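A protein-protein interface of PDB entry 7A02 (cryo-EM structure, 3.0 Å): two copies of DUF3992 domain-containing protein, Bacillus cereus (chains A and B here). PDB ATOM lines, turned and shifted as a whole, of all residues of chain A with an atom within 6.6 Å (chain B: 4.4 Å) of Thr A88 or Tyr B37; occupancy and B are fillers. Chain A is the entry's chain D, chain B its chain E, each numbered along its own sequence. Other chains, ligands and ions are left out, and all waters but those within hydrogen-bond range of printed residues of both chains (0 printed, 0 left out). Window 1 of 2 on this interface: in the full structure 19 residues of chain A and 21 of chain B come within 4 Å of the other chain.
Of chain B, only Tyr B37, Ala B38, Asp B39 and Asn B40 come within 4 Å of Thr A88.
Tyr B37 touches just these residues of chain A: Ser A86, Phe A87 and Thr A88.
Of the printed residues of chain A, Asp B39 touches Glu A75 (3.1 Å) and Thr A88 (3.0 Å).
Of the printed residues of chain A, Ile B35 touches Ala A85.
Of the printed residues of chain B, Ala A85 touches Ile B35 and Ile B36.
Printed residues of chain A within 4 Å of Ala B38: Glu A75, Ile A77, Ser A86, Phe A87 and Thr A88.
Printed residues of chain A within 4 Å of Ile B41: Arg A90.
Met B110 touches none of the printed residues of chain A.
The nearest residue of chain A that does not touch Tyr B37 is Ala A85 (5.1 Å).
The nearest printed residue of chain B that does not touch Arg A90 is Asp B39 (6.8 Å).
Of the 13 printed residues of chain A, 8 touch a printed residue of chain B.
Printed residues of chain A that touch a printed residue of chain B: Glu A75, Ile A77, Ala A85, Ser A86, Phe A87, Thr A88, Val A89 and Arg A90.
Of the 13 printed residues of chain B, 7 touch a printed residue of chain A.
Hydrophobic or aromatic side chains of chain B that line the printed part of chain A: Tyr B37, Ala B38 and Ile B41.
Among the printed residues, 17 pairs touch across the chains.
Among the printed residues, no Asp or Glu carboxylate lies within 4 Å of a Lys or Arg side-chain nitrogen of the other chain.
The backbone carbonyl oxygen of Ala A47 sits close to the side-chain hydroxyl of Thr A88 (3.3 Å).
The backbone carbonyl oxygen of Ala A47 sits at hydrogen-bond distance from the backbone NH of Val A89 (2.9 Å).
The side-chain hydroxyl (OG) of Ser A48 is in hydrogen-bond range of the side-chain hydroxyl (OG1) of Thr A88 (3.2 Å).
O of Gly A49 sits at hydrogen-bond distance from N of Phe A87 (2.9 Å).
The backbone NH of Ile B36 sits at hydrogen-bond distance from the backbone carbonyl oxygen of Val B95 (2.9 Å).
The backbone carbonyl oxygen (O) of Tyr B37 lies within hydrogen-bond range of the backbone NH (N) of Val B95 (3.0 Å).
The backbone carbonyl oxygen (O) of Ile B36 sits at hydrogen-bond distance from the backbone NH (N) of Ser A86 (3.1 Å).
The backbone carbonyl oxygen (O) of Ser A86 sits at hydrogen-bond distance from the backbone NH (N) of Ala B38, at 3.3 Å.
N of Thr A88 lies within hydrogen-bond range of O of Ala B38 (3.3 Å).
O of Arg A90 lies within hydrogen-bond range of ND2 of Asn B40 (3.1 Å).
OE1 of Glu A75 sits close to O of Asp B39 (3.1 Å).
No position is printed for both chains.
Of the 17 pairs that touch across the chains among the printed residues, none has its exchanged pair printed and touching as well.
Ala B38 touches Glu A75.
CD1 of Ile A77 touches CB of Ala B38, at 3.8 Å.
Ile B35 touches Ala A85.
Ala A85 touches Ile B36 (CA to O, 3.7 Å).
Ser A86 touches Tyr B37.
Phe A87 touches Tyr B37 (N to CD1, 3.8 Å).
Phe A87 touches Ala B38.
Tyr B37 touches Thr A88.
Thr A88 touches Asp B39 (O to CB, 3.0 Å).
Asn B40 touches Val A89.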
ATOM      1  N   TYR A  46      35.618  21.182   7.982  1.00  0.00           N
ATOM      2  CA  TYR A  46      34.257  21.167   8.495  1.00  0.00           C
ATOM      3  C   TYR A  46      34.269  20.347   9.770  1.00  0.00           C
ATOM      4  O   TYR A  46      34.721  19.200   9.759  1.00  0.00           O
ATOM      5  CB  TYR A  46      33.290  20.568   7.479  1.00  0.00           C
ATOM      6  CG  TYR A  46      33.011  21.458   6.300  1.00  0.00           C
ATOM      7  CD1 TYR A  46      33.942  21.609   5.292  1.00  0.00           C
ATOM      8  CD2 TYR A  46      31.812  22.133   6.185  1.00  0.00           C
ATOM      9  CE1 TYR A  46      33.695  22.417   4.216  1.00  0.00           C
ATOM     10  CE2 TYR A  46      31.556  22.941   5.111  1.00  0.00           C
ATOM     11  CZ  TYR A  46      32.501  23.078   4.130  1.00  0.00           C
ATOM     12  OH  TYR A  46      32.254  23.886   3.051  1.00  0.00           O
ATOM     13  N   ALA A  47      33.786  20.923  10.861  1.00  0.00           N
ATOM     14  CA  ALA A  47      33.872  20.263  12.151  1.00  0.00           C
ATOM     15  C   ALA A  47      32.527  20.290  12.849  1.00  0.00           C
ATOM     16  O   ALA A  47      31.867  21.327  12.895  1.00  0.00           O
ATOM     17  CB  ALA A  47      34.925  20.923  13.028  1.00  0.00           C
ATOM     18  N   SER A  48      32.135  19.149  13.405  1.00  0.00           N
ATOM     19  CA  SER A  48      30.925  19.023  14.200  1.00  0.00           C
ATOM     20  C   SER A  48      31.285  18.451  15.559  1.00  0.00           C
ATOM     21  O   SER A  48      32.236  17.681  15.685  1.00  0.00           O
ATOM     22  CB  SER A  48      29.897  18.118  13.528  1.00  0.00           C
ATOM     23  OG  SER A  48      29.476  18.654  12.291  1.00  0.00           O
ATOM     24  N   GLY A  49      30.525  18.830  16.577  1.00  0.00           N
ATOM     25  CA  GLY A  49      30.794  18.297  17.898  1.00  0.00           C
ATOM     26  C   GLY A  49      29.955  18.942  18.973  1.00  0.00           C
ATOM     27  O   GLY A  49      28.954  19.597  18.688  1.00  0.00           O
ATOM     28  N   GLU A  75      32.244  32.269  15.394  1.00  0.00           N
ATOM     29  CA  GLU A  75      31.227  31.633  16.218  1.00  0.00           C
ATOM     30  C   GLU A  75      31.564  31.819  17.688  1.00  0.00           C
ATOM     31  O   GLU A  75      32.737  31.798  18.067  1.00  0.00           O
ATOM     32  CB  GLU A  75      31.106  30.144  15.904  1.00  0.00           C
ATOM     33  CG  GLU A  75      30.125  29.823  14.814  1.00  0.00           C
ATOM     34  CD  GLU A  75      28.717  29.750  15.332  1.00  0.00           C
ATOM     35  OE1 GLU A  75      27.917  30.651  15.013  1.00  0.00           O
ATOM     36  OE2 GLU A  75      28.409  28.793  16.065  1.00  0.00           O
ATOM     37  N   ILE A  77      29.713  30.695  21.642  1.00  0.00           N
ATOM     38  CA  ILE A  77      28.639  30.051  22.390  1.00  0.00           C
ATOM     39  C   ILE A  77      28.936  30.158  23.879  1.00  0.00           C
ATOM     40  O   ILE A  77      30.090  30.025  24.301  1.00  0.00           O
ATOM     41  CB  ILE A  77      28.464  28.576  21.979  1.00  0.00           C
ATOM     42  CG1 ILE A  77      28.076  28.467  20.511  1.00  0.00           C
ATOM     43  CG2 ILE A  77      27.383  27.921  22.796  1.00  0.00           C
ATOM     44  CD1 ILE A  77      28.138  27.063  19.981  1.00  0.00           C
ATOM     45  N   SER A  84      24.984  21.248  27.980  1.00  0.00           N
ATOM     46  CA  SER A  84      25.869  21.036  26.848  1.00  0.00           C
ATOM     47  C   SER A  84      25.410  21.891  25.678  1.00  0.00           C
ATOM     48  O   SER A  84      24.321  22.465  25.691  1.00  0.00           O
ATOM     49  CB  SER A  84      25.903  19.563  26.438  1.00  0.00           C
ATOM     50  OG  SER A  84      26.445  18.764  27.467  1.00  0.00           O
ATOM     51  N   ALA A  85      26.258  21.972  24.656  1.00  0.00           N
ATOM     52  CA  ALA A  85      25.889  22.681  23.437  1.00  0.00           C
ATOM     53  C   ALA A  85      26.676  22.125  22.264  1.00  0.00           C
ATOM     54  O   ALA A  85      27.881  21.907  22.382  1.00  0.00           O
ATOM     55  CB  ALA A  85      26.141  24.181  23.572  1.00  0.00           C
ATOM     56  N   SER A  86      26.009  21.925  21.135  1.00  0.00           N
ATOM     57  CA  SER A  86      26.618  21.326  19.958  1.00  0.00           C
ATOM     58  C   SER A  86      26.792  22.362  18.856  1.00  0.00           C
ATOM     59  O   SER A  86      26.284  23.479  18.938  1.00  0.00           O
ATOM     60  CB  SER A  86      25.778  20.150  19.463  1.00  0.00           C
ATOM     61  OG  SER A  86      24.455  20.565  19.205  1.00  0.00           O
ATOM     62  N   PHE A  87      27.530  21.979  17.815  1.00  0.00           N
ATOM     63  CA  PHE A  87      27.870  22.924  16.759  1.00  0.00           C
ATOM     64  C   PHE A  87      28.379  22.196  15.523  1.00  0.00           C
ATOM     65  O   PHE A  87      28.789  21.033  15.586  1.00  0.00           O
ATOM     66  CB  PHE A  87      28.930  23.917  17.232  1.00  0.00           C
ATOM     67  CG  PHE A  87      30.160  23.265  17.781  1.00  0.00           C
ATOM     68  CD1 PHE A  87      31.134  22.767  16.939  1.00  0.00           C
ATOM     69  CD2 PHE A  87      30.343  23.146  19.138  1.00  0.00           C
ATOM     70  CE1 PHE A  87      32.254  22.164  17.439  1.00  0.00           C
ATOM     71  CE2 PHE A  87      31.466  22.548  19.639  1.00  0.00           C
ATOM     72  CZ  PHE A  87      32.421  22.056  18.789  1.00  0.00           C
ATOM     73  N   THR A  88      28.369  22.921  14.400  1.00  0.00           N
ATOM     74  CA  THR A  88      29.141  22.587  13.206  1.00  0.00           C
ATOM     75  C   THR A  88      29.601  23.883  12.551  1.00  0.00           C
ATOM     76  O   THR A  88      28.821  24.826  12.420  1.00  0.00           O
ATOM     77  CB  THR A  88      28.342  21.739  12.211  1.00  0.00           C
ATOM     78  OG1 THR A  88      29.116  21.542  11.024  1.00  0.00           O
ATOM     79  CG2 THR A  88      27.074  22.419  11.829  1.00  0.00           C
ATOM     80  N   VAL A  89      30.871  23.931  12.160  1.00  0.00           N
ATOM     81  CA  VAL A  89      31.530  25.163  11.740  1.00  0.00           C
ATOM     82  C   VAL A  89      32.516  24.844  10.622  1.00  0.00           C
ATOM     83  O   VAL A  89      33.073  23.745  10.557  1.00  0.00           O
ATOM     84  CB  VAL A  89      32.243  25.846  12.933  1.00  0.00           C
ATOM     85  CG1 VAL A  89      33.018  27.059  12.503  1.00  0.00           C
ATOM     86  CG2 VAL A  89      31.245  26.254  13.983  1.00  0.00           C
ATOM     87  N   ARG A  90      32.727  25.811   9.727  1.00  0.00           N
ATOM     88  CA  ARG A  90      33.744  25.705   8.691  1.00  0.00           C
ATOM     89  C   ARG A  90      34.614  26.953   8.701  1.00  0.00           C
ATOM     90  O   ARG A  90      34.234  27.990   9.243  1.00  0.00           O
ATOM     91  CB  ARG A  90      33.147  25.564   7.300  1.00  0.00           C
ATOM     92  CG  ARG A  90      32.356  26.759   6.885  1.00  0.00           C
ATOM     93  CD  ARG A  90      31.994  26.669   5.439  1.00  0.00           C
ATOM     94  NE  ARG A  90      31.330  27.886   4.997  1.00  0.00           N
ATOM     95  CZ  ARG A  90      30.189  27.930   4.329  1.00  0.00           C
ATOM     96  NH1 ARG A  90      29.572  26.815   3.976  1.00  0.00           N
ATOM     97  NH2 ARG A  90      29.681  29.100   3.985  1.00  0.00           N
ATOM     98  N   ILE B  35      21.160  28.641  24.266  1.00  0.00           N
ATOM     99  CA  ILE B  35      21.640  28.153  22.980  1.00  0.00           C
ATOM    100  C   ILE B  35      22.035  26.692  23.111  1.00  0.00           C
ATOM    101  O   ILE B  35      22.840  26.323  23.973  1.00  0.00           O
ATOM    102  CB  ILE B  35      22.823  28.997  22.489  1.00  0.00           C
ATOM    103  CG1 ILE B  35      22.459  30.475  22.480  1.00  0.00           C
ATOM    104  CG2 ILE B  35      23.246  28.555  21.109  1.00  0.00           C
ATOM    105  CD1 ILE B  35      21.529  30.859  21.366  1.00  0.00           C
ATOM    106  N   ILE B  36      21.484  25.855  22.242  1.00  0.00           N
ATOM    107  CA  ILE B  36      21.741  24.423  22.273  1.00  0.00           C
ATOM    108  C   ILE B  36      22.491  23.952  21.038  1.00  0.00           C
ATOM    109  O   ILE B  36      23.064  22.853  21.057  1.00  0.00           O
ATOM    110  CB  ILE B  36      20.423  23.638  22.449  1.00  0.00           C
ATOM    111  CG1 ILE B  36      20.639  22.143  22.560  1.00  0.00           C
ATOM    112  CG2 ILE B  36      19.515  23.880  21.292  1.00  0.00           C
ATOM    113  CD1 ILE B  36      19.363  21.405  22.818  1.00  0.00           C
ATOM    114  N   TYR B  37      22.558  24.768  19.988  1.00  0.00           N
ATOM    115  CA  TYR B  37      23.231  24.407  18.751  1.00  0.00           C
ATOM    116  C   TYR B  37      23.470  25.670  17.940  1.00  0.00           C
ATOM    117  O   TYR B  37      22.644  26.581  17.958  1.00  0.00           O
ATOM    118  CB  TYR B  37      22.391  23.412  17.951  1.00  0.00           C
ATOM    119  CG  TYR B  37      22.965  23.064  16.611  1.00  0.00           C
ATOM    120  CD1 TYR B  37      23.958  22.116  16.488  1.00  0.00           C
ATOM    121  CD2 TYR B  37      22.509  23.679  15.466  1.00  0.00           C
ATOM    122  CE1 TYR B  37      24.479  21.796  15.270  1.00  0.00           C
ATOM    123  CE2 TYR B  37      23.027  23.365  14.247  1.00  0.00           C
ATOM    124  CZ  TYR B  37      24.010  22.425  14.156  1.00  0.00           C
ATOM    125  OH  TYR B  37      24.520  22.109  12.932  1.00  0.00           O
ATOM    126  N   ALA B  38      24.596  25.719  17.233  1.00  0.00           N
ATOM    127  CA  ALA B  38      24.935  26.889  16.437  1.00  0.00           C
ATOM    128  C   ALA B  38      25.892  26.491  15.329  1.00  0.00           C
ATOM    129  O   ALA B  38      26.712  25.590  15.495  1.00  0.00           O
ATOM    130  CB  ALA B  38      25.560  27.985  17.295  1.00  0.00           C
ATOM    131  N   ASP B  39      25.794  27.183  14.199  1.00  0.00           N
ATOM    132  CA  ASP B  39      26.656  26.907  13.060  1.00  0.00           C
ATOM    133  C   ASP B  39      26.914  28.199  12.304  1.00  0.00           C
ATOM    134  O   ASP B  39      26.445  29.272  12.685  1.00  0.00           O
ATOM    135  CB  ASP B  39      26.038  25.860  12.136  1.00  0.00           C
ATOM    136  CG  ASP B  39      24.738  26.318  11.532  1.00  0.00           C
ATOM    137  OD1 ASP B  39      24.268  25.679  10.577  1.00  0.00           O
ATOM    138  OD2 ASP B  39      24.173  27.311  12.016  1.00  0.00           O
ATOM    139  N   ASN B  40      27.669  28.086  11.217  1.00  0.00           N
ATOM    140  CA  ASN B  40      27.841  29.190  10.296  1.00  0.00           C
ATOM    141  C   ASN B  40      27.635  28.781   8.848  1.00  0.00           C
ATOM    142  O   ASN B  40      27.811  29.614   7.957  1.00  0.00           O
ATOM    143  CB  ASN B  40      29.230  29.823  10.459  1.00  0.00           C
ATOM    144  CG  ASN B  40      30.340  28.872  10.126  1.00  0.00           C
ATOM    145  OD1 ASN B  40      30.108  27.696   9.892  1.00  0.00           O
ATOM    146  ND2 ASN B  40      31.563  29.375  10.108  1.00  0.00           N
ATOM    147  N   ILE B  41      27.267  27.530   8.584  1.00  0.00           N
ATOM    148  CA  ILE B  41      26.913  27.111   7.237  1.00  0.00           C
ATOM    149  C   ILE B  41      25.400  27.195   7.091  1.00  0.00           C
ATOM    150  O   ILE B  41      24.721  26.174   6.959  1.00  0.00           O
ATOM    151  CB  ILE B  41      27.414  25.688   6.953  1.00  0.00           C
ATOM    152  CG1 ILE B  41      27.073  24.754   8.105  1.00  0.00           C
ATOM    153  CG2 ILE B  41      28.908  25.680   6.856  1.00  0.00           C
ATOM    154  CD1 ILE B  41      27.377  23.317   7.809  1.00  0.00           C
ATOM    155  N   ILE B  45      22.144  23.546   4.705  1.00  0.00           N
ATOM    156  CA  ILE B  45      22.155  22.624   5.828  1.00  0.00           C
ATOM    157  C   ILE B  45      20.768  22.018   5.949  1.00  0.00           C
ATOM    158  O   ILE B  45      19.759  22.710   5.814  1.00  0.00           O
ATOM    159  CB  ILE B  45      22.606  23.329   7.127  1.00  0.00           C
ATOM    160  CG1 ILE B  45      22.853  22.304   8.222  1.00  0.00           C
ATOM    161  CG2 ILE B  45      21.595  24.351   7.573  1.00  0.00           C
ATOM    162  CD1 ILE B  45      23.586  22.856   9.396  1.00  0.00           C
ATOM    163  N   PHE B  92      18.719  27.174   8.932  1.00  0.00           N
ATOM    164  CA  PHE B  92      18.637  27.731  10.270  1.00  0.00           C
ATOM    165  C   PHE B  92      20.040  28.019  10.775  1.00  0.00           C
ATOM    166  O   PHE B  92      21.018  27.423  10.325  1.00  0.00           O
ATOM    167  CB  PHE B  92      17.906  26.795  11.235  1.00  0.00           C
ATOM    168  CG  PHE B  92      18.559  25.464  11.402  1.00  0.00           C
ATOM    169  CD1 PHE B  92      18.290  24.435  10.533  1.00  0.00           C
ATOM    170  CD2 PHE B  92      19.434  25.241  12.439  1.00  0.00           C
ATOM    171  CE1 PHE B  92      18.888  23.217  10.685  1.00  0.00           C
ATOM    172  CE2 PHE B  92      20.033  24.025  12.595  1.00  0.00           C
ATOM    173  CZ  PHE B  92      19.760  23.012  11.717  1.00  0.00           C
ATOM    174  N   THR B  94      20.694  29.100  14.524  1.00  0.00           N
ATOM    175  CA  THR B  94      20.859  28.688  15.911  1.00  0.00           C
ATOM    176  C   THR B  94      19.617  27.937  16.358  1.00  0.00           C
ATOM    177  O   THR B  94      18.574  27.978  15.708  1.00  0.00           O
ATOM    178  CB  THR B  94      21.096  29.876  16.846  1.00  0.00           C
ATOM    179  OG1 THR B  94      20.003  30.790  16.739  1.00  0.00           O
ATOM    180  CG2 THR B  94      22.379  30.596  16.500  1.00  0.00           C
ATOM    181  N   VAL B  95      19.739  27.234  17.478  1.00  0.00           N
ATOM    182  CA  VAL B  95      18.608  26.587  18.129  1.00  0.00           C
ATOM    183  C   VAL B  95      18.635  26.957  19.601  1.00  0.00           C
ATOM    184  O   VAL B  95      19.698  26.947  20.229  1.00  0.00           O
ATOM    185  CB  VAL B  95      18.636  25.056  17.958  1.00  0.00           C
ATOM    186  CG1 VAL B  95      17.334  24.463  18.420  1.00  0.00           C
ATOM    187  CG2 VAL B  95      18.891  24.684  16.524  1.00  0.00           C
ATOM    188  N   MET B 110      20.678  14.872  16.648  1.00  0.00           N
ATOM    189  CA  MET B 110      20.500  15.518  15.355  1.00  0.00           C
ATOM    190  C   MET B 110      21.520  15.011  14.346  1.00  0.00           C
ATOM    191  O   MET B 110      22.713  14.945  14.649  1.00  0.00           O
ATOM    192  CB  MET B 110      20.616  17.034  15.497  1.00  0.00           C
ATOM    193  CG  MET B 110      20.687  17.773  14.190  1.00  0.00           C
ATOM    194  SD  MET B 110      20.980  19.532  14.407  1.00  0.00           S
ATOM    195  CE  MET B 110      19.384  20.049  14.998  1.00  0.00           C
ATOM    196  N   ILE B 112      23.029  15.810  10.466  1.00  0.00           N
ATOM    197  CA  ILE B 112      23.227  17.023   9.686  1.00  0.00           C
ATOM    198  C   ILE B 112      23.780  16.650   8.322  1.00  0.00           C
ATOM    199  O   ILE B 112      24.755  15.901   8.232  1.00  0.00           O
ATOM    200  CB  ILE B 112      24.184  17.988  10.401  1.00  0.00           C
ATOM    201  CG1 ILE B 112      23.661  18.305  11.796  1.00  0.00           C
ATOM    202  CG2 ILE B 112      24.366  19.243   9.603  1.00  0.00           C
ATOM    203  CD1 ILE B 112      24.740  18.640  12.777  1.00  0.00           C
